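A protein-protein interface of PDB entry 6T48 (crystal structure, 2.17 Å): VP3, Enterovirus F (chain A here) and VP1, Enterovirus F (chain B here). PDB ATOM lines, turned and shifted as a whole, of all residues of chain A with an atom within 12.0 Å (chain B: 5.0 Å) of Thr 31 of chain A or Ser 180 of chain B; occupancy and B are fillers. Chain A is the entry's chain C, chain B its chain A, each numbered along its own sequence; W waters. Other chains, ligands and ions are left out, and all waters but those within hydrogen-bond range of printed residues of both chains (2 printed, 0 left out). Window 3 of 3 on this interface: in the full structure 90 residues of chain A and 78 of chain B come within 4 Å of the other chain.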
ATOM      1  N   LEU A  25       4.667  15.603  18.341  1.00  0.00           N
ATOM      2  CA  LEU A  25       3.896  14.431  17.914  1.00  0.00           C
ATOM      3  C   LEU A  25       2.604  14.939  17.276  1.00  0.00           C
ATOM      4  O   LEU A  25       1.542  14.919  17.896  1.00  0.00           O
ATOM      5  CB  LEU A  25       3.563  13.559  19.128  1.00  0.00           C
ATOM      6  CG  LEU A  25       4.744  13.112  19.990  1.00  0.00           C
ATOM      7  CD1 LEU A  25       4.232  12.402  21.229  1.00  0.00           C
ATOM      8  CD2 LEU A  25       5.649  12.198  19.181  1.00  0.00           C
ATOM      9  N   LYS A  27       0.422  13.743  15.152  1.00  0.00           N
ATOM     10  CA  LYS A  27      -0.756  12.891  15.014  1.00  0.00           C
ATOM     11  C   LYS A  27      -1.187  12.203  16.301  1.00  0.00           C
ATOM     12  O   LYS A  27      -2.103  11.384  16.299  1.00  0.00           O
ATOM     13  CB  LYS A  27      -0.521  11.863  13.903  1.00  0.00           C
ATOM     14  CG  LYS A  27      -0.312  12.526  12.544  1.00  0.00           C
ATOM     15  CD  LYS A  27      -0.070  11.527  11.441  1.00  0.00           C
ATOM     16  CE  LYS A  27       0.194  12.244  10.127  1.00  0.00           C
ATOM     17  NZ  LYS A  27      -0.953  13.115   9.752  1.00  0.00           N
ATOM     18  N   PHE A  28      -0.538  12.554  17.405  1.00  0.00           N
ATOM     19  CA  PHE A  28      -0.856  11.963  18.702  1.00  0.00           C
ATOM     20  C   PHE A  28      -2.305  12.216  19.107  1.00  0.00           C
ATOM     21  O   PHE A  28      -2.843  13.301  18.894  1.00  0.00           O
ATOM     22  CB  PHE A  28       0.067  12.538  19.772  1.00  0.00           C
ATOM     23  CG  PHE A  28      -0.126  11.929  21.127  1.00  0.00           C
ATOM     24  CD1 PHE A  28       0.510  10.740  21.466  1.00  0.00           C
ATOM     25  CD2 PHE A  28      -0.927  12.557  22.073  1.00  0.00           C
ATOM     26  CE1 PHE A  28       0.356  10.186  22.733  1.00  0.00           C
ATOM     27  CE2 PHE A  28      -1.090  12.013  23.342  1.00  0.00           C
ATOM     28  CZ  PHE A  28      -0.446  10.825  23.675  1.00  0.00           C
ATOM     29  N   GLN A  29      -2.926  11.203  19.703  1.00  0.00           N
ATOM     30  CA  GLN A  29      -4.308  11.292  20.160  1.00  0.00           C
ATOM     31  C   GLN A  29      -4.349  10.935  21.647  1.00  0.00           C
ATOM     32  O   GLN A  29      -4.209   9.773  22.029  1.00  0.00           O
ATOM     33  CB  GLN A  29      -5.181  10.346  19.334  1.00  0.00           C
ATOM     34  CG  GLN A  29      -5.190  10.724  17.852  1.00  0.00           C
ATOM     35  CD  GLN A  29      -5.805   9.661  16.962  1.00  0.00           C
ATOM     36  OE1 GLN A  29      -5.304   8.540  16.871  1.00  0.00           O
ATOM     37  NE2 GLN A  29      -6.895  10.011  16.295  1.00  0.00           N
ATOM     38  N   PRO A  30      -4.535  11.945  22.507  1.00  0.00           N
ATOM     39  CA  PRO A  30      -4.589  11.789  23.965  1.00  0.00           C
ATOM     40  C   PRO A  30      -5.694  10.895  24.510  1.00  0.00           C
ATOM     41  O   PRO A  30      -6.685  10.629  23.834  1.00  0.00           O
ATOM     42  CB  PRO A  30      -4.715  13.233  24.454  1.00  0.00           C
ATOM     43  CG  PRO A  30      -5.477  13.887  23.357  1.00  0.00           C
ATOM     44  CD  PRO A  30      -4.792  13.346  22.127  1.00  0.00           C
ATOM     45  N   THR A  31      -5.505  10.424  25.739  1.00  0.00           N
ATOM     46  CA  THR A  31      -6.505   9.588  26.391  1.00  0.00           C
ATOM     47  C   THR A  31      -7.741  10.455  26.592  1.00  0.00           C
ATOM     48  O   THR A  31      -7.644  11.680  26.670  1.00  0.00           O
ATOM     49  CB  THR A  31      -6.030   9.109  27.772  1.00  0.00           C
ATOM     50  OG1 THR A  31      -5.613  10.240  28.547  1.00  0.00           O
ATOM     51  CG2 THR A  31      -4.876   8.132  27.637  1.00  0.00           C
ATOM     52  N   PRO A  32      -8.922   9.835  26.678  1.00  0.00           N
ATOM     53  CA  PRO A  32     -10.140  10.623  26.872  1.00  0.00           C
ATOM     54  C   PRO A  32     -10.199  11.314  28.225  1.00  0.00           C
ATOM     55  O   PRO A  32      -9.575  10.872  29.193  1.00  0.00           O
ATOM     56  CB  PRO A  32     -11.247   9.585  26.719  1.00  0.00           C
ATOM     57  CG  PRO A  32     -10.603   8.338  27.239  1.00  0.00           C
ATOM     58  CD  PRO A  32      -9.233   8.397  26.599  1.00  0.00           C
ATOM     59  N   VAL A  33     -10.940  12.413  28.282  1.00  0.00           N
ATOM     60  CA  VAL A  33     -11.119  13.134  29.531  1.00  0.00           C
ATOM     61  C   VAL A  33     -12.213  12.359  30.248  1.00  0.00           C
ATOM     62  O   VAL A  33     -13.291  12.161  29.694  1.00  0.00           O
ATOM     63  CB  VAL A  33     -11.622  14.567  29.298  1.00  0.00           C
ATOM     64  CG1 VAL A  33     -11.911  15.231  30.632  1.00  0.00           C
ATOM     65  CG2 VAL A  33     -10.592  15.362  28.521  1.00  0.00           C
ATOM     66  N   ILE A  34     -11.944  11.898  31.462  1.00  0.00           N
ATOM     67  CA  ILE A  34     -12.963  11.155  32.184  1.00  0.00           C
ATOM     68  C   ILE A  34     -13.576  12.023  33.265  1.00  0.00           C
ATOM     69  O   ILE A  34     -13.095  13.123  33.540  1.00  0.00           O
ATOM     70  CB  ILE A  34     -12.400   9.863  32.823  1.00  0.00           C
ATOM     71  CG1 ILE A  34     -11.331  10.207  33.861  1.00  0.00           C
ATOM     72  CG2 ILE A  34     -11.834   8.957  31.737  1.00  0.00           C
ATOM     73  CD1 ILE A  34     -10.803   8.997  34.612  1.00  0.00           C
ATOM     74  N   ASP A  35     -14.648  11.525  33.866  1.00  0.00           N
ATOM     75  CA  ASP A  35     -15.344  12.244  34.917  1.00  0.00           C
ATOM     76  C   ASP A  35     -14.604  12.148  36.247  1.00  0.00           C
ATOM     77  O   ASP A  35     -14.554  11.085  36.866  1.00  0.00           O
ATOM     78  CB  ASP A  35     -16.763  11.688  35.068  1.00  0.00           C
ATOM     79  CG  ASP A  35     -17.510  12.304  36.232  1.00  0.00           C
ATOM     80  OD1 ASP A  35     -17.536  13.548  36.327  1.00  0.00           O
ATOM     81  OD2 ASP A  35     -18.076  11.543  37.047  1.00  0.00           O
ATOM     82  N   ILE A  36     -14.018  13.263  36.671  1.00  0.00           N
ATOM     83  CA  ILE A  36     -13.298  13.323  37.938  1.00  0.00           C
ATOM     84  C   ILE A  36     -13.921  14.438  38.769  1.00  0.00           C
ATOM     85  O   ILE A  36     -14.075  15.562  38.296  1.00  0.00           O
ATOM     86  CB  ILE A  36     -11.804  13.657  37.743  1.00  0.00           C
ATOM     87  CG1 ILE A  36     -11.155  12.644  36.802  1.00  0.00           C
ATOM     88  CG2 ILE A  36     -11.089  13.651  39.096  1.00  0.00           C
ATOM     89  CD1 ILE A  36      -9.704  12.954  36.503  1.00  0.00           C
ATOM     90  N   ARG B 109      -4.510  17.986  33.307  1.00  0.00           N
ATOM     91  CA  ARG B 109      -4.221  17.625  31.927  1.00  0.00           C
ATOM     92  C   ARG B 109      -3.737  18.910  31.293  1.00  0.00           C
ATOM     93  O   ARG B 109      -4.285  19.982  31.552  1.00  0.00           O
ATOM     94  CB  ARG B 109      -5.473  17.194  31.162  1.00  0.00           C
ATOM     95  CG  ARG B 109      -6.027  15.843  31.496  1.00  0.00           C
ATOM     96  CD  ARG B 109      -7.337  15.648  30.754  1.00  0.00           C
ATOM     97  NE  ARG B 109      -7.164  15.557  29.305  1.00  0.00           N
ATOM     98  CZ  ARG B 109      -7.095  14.412  28.630  1.00  0.00           C
ATOM     99  NH1 ARG B 109      -6.939  14.424  27.313  1.00  0.00           N
ATOM    100  NH2 ARG B 109      -7.188  13.253  29.269  1.00  0.00           N
ATOM    101  N   PHE B 177      -0.809  16.122  25.700  1.00  0.00           N
ATOM    102  CA  PHE B 177      -0.973  15.474  26.995  1.00  0.00           C
ATOM    103  C   PHE B 177      -0.651  14.007  26.711  1.00  0.00           C
ATOM    104  O   PHE B 177      -1.463  13.286  26.132  1.00  0.00           O
ATOM    105  CB  PHE B 177      -2.411  15.618  27.494  1.00  0.00           C
ATOM    106  CG  PHE B 177      -2.697  14.795  28.708  1.00  0.00           C
ATOM    107  CD1 PHE B 177      -2.010  15.031  29.895  1.00  0.00           C
ATOM    108  CD2 PHE B 177      -3.593  13.736  28.647  1.00  0.00           C
ATOM    109  CE1 PHE B 177      -2.208  14.216  31.005  1.00  0.00           C
ATOM    110  CE2 PHE B 177      -3.798  12.915  29.750  1.00  0.00           C
ATOM    111  CZ  PHE B 177      -3.103  13.154  30.930  1.00  0.00           C
ATOM    112  N   MET B 178       0.531  13.571  27.135  1.00  0.00           N
ATOM    113  CA  MET B 178       1.016  12.225  26.841  1.00  0.00           C
ATOM    114  C   MET B 178       0.851  11.076  27.824  1.00  0.00           C
ATOM    115  O   MET B 178       1.188   9.941  27.491  1.00  0.00           O
ATOM    116  CB  MET B 178       2.494  12.320  26.474  1.00  0.00           C
ATOM    117  CG  MET B 178       2.761  13.106  25.208  1.00  0.00           C
ATOM    118  SD  MET B 178       4.483  13.579  25.103  1.00  0.00           S
ATOM    119  CE  MET B 178       5.259  11.983  24.923  1.00  0.00           C
ATOM    120  N   SER B 179       0.341  11.338  29.019  1.00  0.00           N
ATOM    121  CA  SER B 179       0.203  10.265  29.995  1.00  0.00           C
ATOM    122  C   SER B 179      -0.717   9.131  29.562  1.00  0.00           C
ATOM    123  O   SER B 179      -1.651   9.325  28.778  1.00  0.00           O
ATOM    124  CB  SER B 179      -0.293  10.818  31.331  1.00  0.00           C
ATOM    125  OG  SER B 179      -0.360   9.789  32.304  1.00  0.00           O
ATOM    126  N   SER B 180      -0.428   7.941  30.076  1.00  0.00           N
ATOM    127  CA  SER B 180      -1.238   6.762  29.800  1.00  0.00           C
ATOM    128  C   SER B 180      -2.494   6.904  30.654  1.00  0.00           C
ATOM    129  O   SER B 180      -3.499   6.240  30.416  1.00  0.00           O
ATOM    130  CB  SER B 180      -0.481   5.491  30.190  1.00  0.00           C
ATOM    131  OG  SER B 180      -0.096   5.524  31.555  1.00  0.00           O
ATOM    132  N   ALA B 181      -2.418   7.778  31.656  1.00  0.00           N
ATOM    133  CA  ALA B 181      -3.544   8.046  32.550  1.00  0.00           C
ATOM    134  C   ALA B 181      -4.423   9.113  31.902  1.00  0.00           C
ATOM    135  O   ALA B 181      -4.096   9.619  30.832  1.00  0.00           O
ATOM    136  CB  ALA B 181      -3.033   8.544  33.900  1.00  0.00           C
ATOM    137  N   ASN B 182      -5.531   9.465  32.546  1.00  0.00           N
ATOM    138  CA  ASN B 182      -6.418  10.478  31.988  1.00  0.00           C
ATOM    139  C   ASN B 182      -6.093  11.870  32.514  1.00  0.00           C
ATOM    140  O   ASN B 182      -6.776  12.846  32.205  1.00  0.00           O
ATOM    141  CB  ASN B 182      -7.869  10.103  32.272  1.00  0.00           C
ATOM    142  CG  ASN B 182      -8.201   8.715  31.768  1.00  0.00           C
ATOM    143  OD1 ASN B 182      -7.978   7.722  32.459  1.00  0.00           O
ATOM    144  ND2 ASN B 182      -8.704   8.635  30.540  1.00  0.00           N
ATOM    145  N   SER B 207       3.616   6.724  35.455  1.00  0.00           N
ATOM    146  CA  SER B 207       3.025   7.270  34.238  1.00  0.00           C
ATOM    147  C   SER B 207       3.332   8.753  34.020  1.00  0.00           C
ATOM    148  O   SER B 207       3.058   9.295  32.952  1.00  0.00           O
ATOM    149  CB  SER B 207       1.512   7.041  34.242  1.00  0.00           C
ATOM    150  OG  SER B 207       0.934   7.508  35.446  1.00  0.00           O
HETATM  151  O   HOH W   1      -2.697  10.943  26.788  1.00  0.00           O
HETATM  152  O   HOH W   2      -9.623  13.298  32.703  1.00  0.00           O
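Thr 31 of chain A touches six residues of chain B.
Of chain A, only Thr 31 (3.6 Å) comes within 4 Å of Ser 180 of chain B.
Of the printed residues of chain A, Ser 179 of chain B touches Thr 31 (3.6 Å).
Ala 181 of chain B touches just one residue of chain A: Thr 31 (2.8 Å).
Asn 182 of chain B touches just these residues of chain A: Thr 31, Pro 32 and Ile 34.
No residue of chain A comes within 4 Å of Ser 207 of chain B.
Of the printed residues of chain B, Ile 34 of chain A touches Asn 182.
Of the printed residues of chain B, Pro 32 of chain A touches Arg 109 (3.4 Å) and Asn 182 (2.8 Å).
Printed residues of chain B within 4 Å of Val 33 of chain A: Arg 109 (3.5 Å).
Of the printed residues of chain A, Arg 109 of chain B touches Pro 30 (3.8 Å), Thr 31 (2.9 Å), Pro 32 (3.4 Å) and Val 33 (3.5 Å).
Of the printed residues of chain B, Leu 25 of chain A touches Met 178 (3.9 Å).
The nearest printed residue of chain B that does not touch Thr 31 of chain A is Met 178 of chain B (6.3 Å).
The nearest printed residue of chain B that does not touch Ile 34 of chain A is Arg 109 of chain B (5.4 Å).
Met 178 of chain B touches Leu 25 of chain A.
Phe 28 of chain A touches Phe 177 of chain B.
Phe 28 of chain A touches Met 178 of chain B.
CB of Pro 30 of chain A touches NH1 of Arg 109 of chain B, 3.8 Å away.
O of Phe 177 of chain B touches CB of Pro 30 of chain A, at 3.7 Å.
OG1 of Thr 31 of chain A touches CE2 of Phe 177 of chain B (3.4 Å).
Thr 31 of chain A touches Ser 179 of chain B.
O of Ser 180 of chain B touches CG2 of Thr 31 of chain A, at 3.6 Å.
Thr 31 of chain A touches Asn 182 of chain B (OG1 to CA, 3.5 Å).
Asn 182 of chain B touches Ile 34 of chain A.
Water W1 lies within hydrogen-bond range of O of Phe 177 of chain B, O of Ser 179 of chain B and N of Thr 31 of chain A.
Water W2 lies within hydrogen-bond range of O of Asn 182 of chain B (2.9 Å) and N of Ile 34 of chain A (3.0 Å).
NH2 of Arg 109 of chain B is in hydrogen-bond range of O of Asn 182 of chain B.
The side-chain hydroxyl (OG) of Ser 179 of chain B is in hydrogen-bond range of the backbone NH (N) of Ala 181 of chain B (2.9 Å).
Hydrophobic or aromatic side chains of chain A within 4 Å of the printed part of chain B: Leu 25, Phe 28, Pro 30, Pro 32, Val 33 and Ile 34.
Printed residues of chain B that touch a printed residue of chain A: Arg 109, Phe 177, Met 178, Ser 179, Ser 180, Ala 181 and Asn 182.
Hydrophobic or aromatic side chains of chain B that line the printed part of chain A: Phe 177 and Met 178.
Among the printed residues, no Asp or Glu carboxylate lies within 4 Å of a Lys or Arg side-chain nitrogen of the other chain.
OG1 of Thr 31 of chain A lies within hydrogen-bond range of O of Ala 181 of chain B (2.8 Å).
ND2 of Asn 182 of chain B sits at hydrogen-bond distance from O of Pro 32 of chain A, 2.8 Å away.
The backbone carbonyl oxygen of Pro 32 of chain A lies within hydrogen-bond range of the guanidinium group of Arg 109 of chain B.
NH1 of Arg 109 of chain B sits at hydrogen-bond distance from O of Thr 31 of chain A (2.9 Å).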
